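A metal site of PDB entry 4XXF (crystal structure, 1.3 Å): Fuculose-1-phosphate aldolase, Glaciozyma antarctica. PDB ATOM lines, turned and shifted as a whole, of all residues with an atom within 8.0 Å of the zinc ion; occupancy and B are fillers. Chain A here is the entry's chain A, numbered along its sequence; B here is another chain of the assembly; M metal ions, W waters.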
ATOM      1  N   ALA A  43       7.336   6.058   4.686  1.00  0.00           N
ATOM      2  CA  ALA A  43       6.636   4.859   5.058  1.00  0.00           C
ATOM      3  C   ALA A  43       5.774   5.152   6.283  1.00  0.00           C
ATOM      4  O   ALA A  43       6.049   6.079   7.062  1.00  0.00           O
ATOM      5  CB  ALA A  43       7.611   3.733   5.349  1.00  0.00           C
ATOM      6  N   GLY A  44       4.740   4.354   6.465  1.00  0.00           N
ATOM      7  CA  GLY A  44       3.973   4.479   7.677  1.00  0.00           C
ATOM      8  C   GLY A  44       2.638   5.157   7.488  1.00  0.00           C
ATOM      9  O   GLY A  44       2.468   6.136   6.750  1.00  0.00           O
ATOM     10  N   HIS A  45       1.687   4.605   8.211  1.00  0.00           N
ATOM     11  CA  HIS A  45       0.345   5.119   8.180  1.00  0.00           C
ATOM     12  C   HIS A  45      -0.311   4.859   9.512  1.00  0.00           C
ATOM     13  O   HIS A  45      -0.090   3.831  10.156  1.00  0.00           O
ATOM     14  CB  HIS A  45      -0.459   4.489   7.033  1.00  0.00           C
ATOM     15  CG  HIS A  45       0.250   3.367   6.359  1.00  0.00           C
ATOM     16  ND1 HIS A  45       0.151   2.059   6.776  1.00  0.00           N
ATOM     17  CD2 HIS A  45       1.091   3.360   5.292  1.00  0.00           C
ATOM     18  CE1 HIS A  45       0.877   1.290   6.000  1.00  0.00           C
ATOM     19  NE2 HIS A  45       1.470   2.053   5.097  1.00  0.00           N
ATOM     20  N   ASN A  95      -1.065   6.971   0.439  1.00  0.00           N
ATOM     21  CA  ASN A  95      -0.274   5.820   0.046  1.00  0.00           C
ATOM     22  C   ASN A  95      -1.226   4.619  -0.063  1.00  0.00           C
ATOM     23  O   ASN A  95      -1.657   4.080   0.957  1.00  0.00           O
ATOM     24  CB  ASN A  95       0.859   5.609   1.052  1.00  0.00           C
ATOM     25  CG  ASN A  95       1.529   4.247   0.937  1.00  0.00           C
ATOM     26  OD1 ASN A  95       1.374   3.515  -0.049  1.00  0.00           O
ATOM     27  ND2 ASN A  95       2.307   3.893   1.956  1.00  0.00           N
ATOM     28  N   ALA A  97      -1.248   1.309  -1.321  1.00  0.00           N
ATOM     29  CA  ALA A  97      -0.911  -0.050  -0.935  1.00  0.00           C
ATOM     30  C   ALA A  97      -0.913  -0.180   0.588  1.00  0.00           C
ATOM     31  O   ALA A  97      -1.506  -1.104   1.143  1.00  0.00           O
ATOM     32  CB  ALA A  97       0.443  -0.456  -1.500  1.00  0.00           C
ATOM     33  N   GLY A  98      -0.276   0.785   1.235  1.00  0.00           N
ATOM     34  CA  GLY A  98      -0.240   0.845   2.682  1.00  0.00           C
ATOM     35  C   GLY A  98      -1.616   1.005   3.305  1.00  0.00           C
ATOM     36  O   GLY A  98      -1.951   0.323   4.271  1.00  0.00           O
ATOM     37  N   ILE A 101      -3.849  -2.219   3.354  1.00  0.00           N
ATOM     38  CA  ILE A 101      -3.590  -3.127   4.476  1.00  0.00           C
ATOM     39  C   ILE A 101      -4.495  -2.769   5.651  1.00  0.00           C
ATOM     40  O   ILE A 101      -5.144  -3.643   6.258  1.00  0.00           O
ATOM     41  CB  ILE A 101      -2.117  -3.101   4.911  1.00  0.00           C
ATOM     42  CG1 ILE A 101      -1.245  -3.708   3.808  1.00  0.00           C
ATOM     43  CG2 ILE A 101      -1.928  -3.856   6.212  1.00  0.00           C
ATOM     44  CD1 ILE A 101       0.246  -3.598   4.067  1.00  0.00           C
ATOM     45  N   HIS A 102      -4.556  -1.484   5.982  1.00  0.00           N
ATOM     46  CA  HIS A 102      -5.425  -1.043   7.071  1.00  0.00           C
ATOM     47  C   HIS A 102      -6.881  -1.304   6.724  1.00  0.00           C
ATOM     48  O   HIS A 102      -7.656  -1.763   7.556  1.00  0.00           O
ATOM     49  CB  HIS A 102      -5.220   0.441   7.368  1.00  0.00           C
ATOM     50  CG  HIS A 102      -3.890   0.764   7.977  1.00  0.00           C
ATOM     51  ND1 HIS A 102      -3.728   1.710   8.950  1.00  0.00           N
ATOM     52  CD2 HIS A 102      -2.657   0.270   7.716  1.00  0.00           C
ATOM     53  CE1 HIS A 102      -2.452   1.795   9.285  1.00  0.00           C
ATOM     54  NE2 HIS A 102      -1.778   0.930   8.555  1.00  0.00           N
ATOM     55  N   HIS A 117       1.119   1.686  11.795  1.00  0.00           N
ATOM     56  CA  HIS A 117       2.219   1.011  11.145  1.00  0.00           C
ATOM     57  C   HIS A 117       3.309   2.023  10.792  1.00  0.00           C
ATOM     58  O   HIS A 117       3.042   3.098  10.285  1.00  0.00           O
ATOM     59  CB  HIS A 117       1.741   0.311   9.880  1.00  0.00           C
ATOM     60  CG  HIS A 117       2.848  -0.252   9.055  1.00  0.00           C
ATOM     61  ND1 HIS A 117       3.669  -1.272   9.499  1.00  0.00           N
ATOM     62  CD2 HIS A 117       3.285   0.065   7.811  1.00  0.00           C
ATOM     63  CE1 HIS A 117       4.548  -1.563   8.558  1.00  0.00           C
ATOM     64  NE2 HIS A 117       4.351  -0.759   7.524  1.00  0.00           N
ATOM     65  N   SER A 118       4.552   1.666  11.085  1.00  0.00           N
ATOM     66  CA  SER A 118       5.698   2.504  10.754  1.00  0.00           C
ATOM     67  C   SER A 118       6.913   1.615  10.709  1.00  0.00           C
ATOM     68  O   SER A 118       6.939   0.573  11.370  1.00  0.00           O
ATOM     69  CB  SER A 118       5.859   3.612  11.806  1.00  0.00           C
ATOM     70  OG  SER A 118       6.765   4.611  11.377  1.00  0.00           O
ATOM     71  N   HIS A 119       7.916   1.998   9.928  1.00  0.00           N
ATOM     72  CA  HIS A 119       9.107   1.185   9.775  1.00  0.00           C
ATOM     73  C   HIS A 119      10.141   1.573  10.818  1.00  0.00           C
ATOM     74  O   HIS A 119      11.217   2.079  10.504  1.00  0.00           O
ATOM     75  CB  HIS A 119       9.654   1.320   8.359  1.00  0.00           C
ATOM     76  CG  HIS A 119       8.732   0.758   7.316  1.00  0.00           C
ATOM     77  ND1 HIS A 119       9.082   0.649   5.995  1.00  0.00           N
ATOM     78  CD2 HIS A 119       7.465   0.280   7.420  1.00  0.00           C
ATOM     79  CE1 HIS A 119       8.074   0.134   5.314  1.00  0.00           C
ATOM     80  NE2 HIS A 119       7.090  -0.110   6.155  1.00  0.00           N
ATOM     81  N   ILE A 166      -2.179 -10.411   5.596  1.00  0.00           N
ATOM     82  CA  ILE A 166      -1.878  -9.795   6.894  1.00  0.00           C
ATOM     83  C   ILE A 166      -3.090  -9.828   7.831  1.00  0.00           C
ATOM     84  O   ILE A 166      -2.969 -10.172   9.000  1.00  0.00           O
ATOM     85  CB  ILE A 166      -1.380  -8.341   6.716  1.00  0.00           C
ATOM     86  CG1 ILE A 166       0.012  -8.345   6.055  1.00  0.00           C
ATOM     87  CG2 ILE A 166      -1.320  -7.629   8.050  1.00  0.00           C
ATOM     88  CD1 ILE A 166       0.501  -6.986   5.581  1.00  0.00           C
ATOM     89  N   LEU A 178       5.669  -8.347  11.121  1.00  0.00           N
ATOM     90  CA  LEU A 178       5.695  -8.663   9.699  1.00  0.00           C
ATOM     91  C   LEU A 178       7.130  -8.926   9.278  1.00  0.00           C
ATOM     92  O   LEU A 178       7.939  -8.007   9.266  1.00  0.00           O
ATOM     93  CB  LEU A 178       5.096  -7.516   8.895  1.00  0.00           C
ATOM     94  CG  LEU A 178       3.685  -7.085   9.313  1.00  0.00           C
ATOM     95  CD1 LEU A 178       3.352  -5.726   8.697  1.00  0.00           C
ATOM     96  CD2 LEU A 178       2.657  -8.139   8.913  1.00  0.00           C
ATOM     97  N   ASN A 180      10.628  -9.207   7.772  1.00  0.00           N
ATOM     98  CA  ASN A 180      11.355  -8.372   6.810  1.00  0.00           C
ATOM     99  C   ASN A 180      10.665  -7.046   6.526  1.00  0.00           C
ATOM    100  O   ASN A 180      10.805  -6.494   5.438  1.00  0.00           O
ATOM    101  CB  ASN A 180      11.571  -9.097   5.482  1.00  0.00           C
ATOM    102  CG  ASN A 180      12.214 -10.461   5.643  1.00  0.00           C
ATOM    103  OD1 ASN A 180      11.602 -11.485   5.289  1.00  0.00           O
ATOM    104  ND2 ASN A 180      13.437 -10.493   6.144  1.00  0.00           N
ATOM    105  N   HIS A 181       9.908  -6.536   7.488  1.00  0.00           N
ATOM    106  CA  HIS A 181       9.075  -5.376   7.224  1.00  0.00           C
ATOM    107  C   HIS A 181       9.020  -4.493   8.466  1.00  0.00           C
ATOM    108  O   HIS A 181       9.564  -3.389   8.474  1.00  0.00           O
ATOM    109  CB  HIS A 181       7.692  -5.845   6.758  1.00  0.00           C
ATOM    110  CG  HIS A 181       6.775  -4.741   6.324  1.00  0.00           C
ATOM    111  ND1 HIS A 181       5.522  -4.993   5.808  1.00  0.00           N
ATOM    112  CD2 HIS A 181       6.925  -3.398   6.315  1.00  0.00           C
ATOM    113  CE1 HIS A 181       4.930  -3.844   5.511  1.00  0.00           C
ATOM    114  NE2 HIS A 181       5.759  -2.859   5.805  1.00  0.00           N
ATOM    115  N   GLY A 182       8.395  -5.005   9.519  1.00  0.00           N
ATOM    116  CA  GLY A 182       8.279  -4.237  10.743  1.00  0.00           C
ATOM    117  C   GLY A 182       7.011  -4.580  11.496  1.00  0.00           C
ATOM    118  O   GLY A 182       6.510  -5.706  11.409  1.00  0.00           O
ATOM    119  N   LEU A 183       6.486  -3.589  12.197  1.00  0.00           N
ATOM    120  CA  LEU A 183       5.392  -3.805  13.146  1.00  0.00           C
ATOM    121  C   LEU A 183       4.094  -3.168  12.700  1.00  0.00           C
ATOM    122  O   LEU A 183       4.088  -2.102  12.087  1.00  0.00           O
ATOM    123  CB  LEU A 183       5.778  -3.219  14.510  1.00  0.00           C
ATOM    124  CG  LEU A 183       7.137  -3.602  15.073  1.00  0.00           C
ATOM    125  CD1 LEU A 183       7.344  -2.848  16.375  1.00  0.00           C
ATOM    126  CD2 LEU A 183       7.206  -5.091  15.297  1.00  0.00           C
ATOM    127  N   LEU A 184       2.982  -3.787  13.078  1.00  0.00           N
ATOM    128  CA  LEU A 184       1.677  -3.178  12.939  1.00  0.00           C
ATOM    129  C   LEU A 184       0.848  -3.489  14.191  1.00  0.00           C
ATOM    130  O   LEU A 184       0.878  -4.622  14.684  1.00  0.00           O
ATOM    131  CB  LEU A 184       0.982  -3.686  11.668  1.00  0.00           C
ATOM    132  CG  LEU A 184      -0.435  -3.176  11.375  1.00  0.00           C
ATOM    133  CD1 LEU A 184      -0.689  -3.167   9.881  1.00  0.00           C
ATOM    134  CD2 LEU A 184      -1.505  -4.028  12.052  1.00  0.00           C
ATOM    135  N   GLN B 138      12.040  -4.403   3.804  1.00  0.00           N
ATOM    136  CA  GLN B 138      11.417  -3.725   2.685  1.00  0.00           C
ATOM    137  C   GLN B 138      12.221  -2.488   2.287  1.00  0.00           C
ATOM    138  O   GLN B 138      12.511  -2.269   1.108  1.00  0.00           O
ATOM    139  CB  GLN B 138       9.990  -3.357   3.030  1.00  0.00           C
ATOM    140  CG  GLN B 138       9.269  -2.628   1.934  1.00  0.00           C
ATOM    141  CD  GLN B 138       7.803  -2.441   2.256  1.00  0.00           C
ATOM    142  OE1 GLN B 138       7.112  -3.392   2.601  1.00  0.00           O
ATOM    143  NE2 GLN B 138       7.337  -1.202   2.146  1.00  0.00           N
ATOM    144  N   ASP B 139      12.617  -1.687   3.280  1.00  0.00           N
ATOM    145  CA  ASP B 139      13.404  -0.488   3.011  1.00  0.00           C
ATOM    146  C   ASP B 139      14.721  -0.797   2.283  1.00  0.00           C
ATOM    147  O   ASP B 139      15.140  -0.051   1.387  1.00  0.00           O
ATOM    148  CB  ASP B 139      13.700   0.253   4.322  1.00  0.00           C
ATOM    149  CG  ASP B 139      12.429   0.783   5.003  1.00  0.00           C
ATOM    150  OD1 ASP B 139      11.497   1.257   4.310  1.00  0.00           O
ATOM    151  OD2 ASP B 139      12.358   0.759   6.254  1.00  0.00           O
HETATM  152 ZN    ZN M   1       5.192  -0.854   5.618  1.00  0.00          ZN
HETATM  153  O   HOH W   1       3.203  -1.409   4.872  1.00  0.00           O
HETATM  154  O   HOH W   2       5.560  -0.942   3.625  1.00  0.00           O
HETATM  155  O   HOH W   3       4.636   1.174   5.087  1.00  0.00           O
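ND1 of His 119 sits at hydrogen-bond distance from OD1 of Asp 139 of chain B, 3.0 Å away. ND1 of His 117 lies within hydrogen-bond range of O of Leu 183 (2.7 Å). The backbone carbonyl oxygen (O) of His 117 is in hydrogen-bond range of the backbone NH (N) of His 45 (2.9 Å).
The zinc ion is bound by water W2 (2.0 Å), NE2 of His 117 (2.1 Å), NE2 of His 181 (2.1 Å), NE2 of His 119 (2.1 Å), water W3 (2.2 Å) and water W1 (2.2 Å). The zinc ion has six donor atoms within binding distance.
Water W3 bridges NE2 of His 45 and N of Gly 44.
Of the 20 residues printed, 3 come within 4 Å of the zinc ion.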
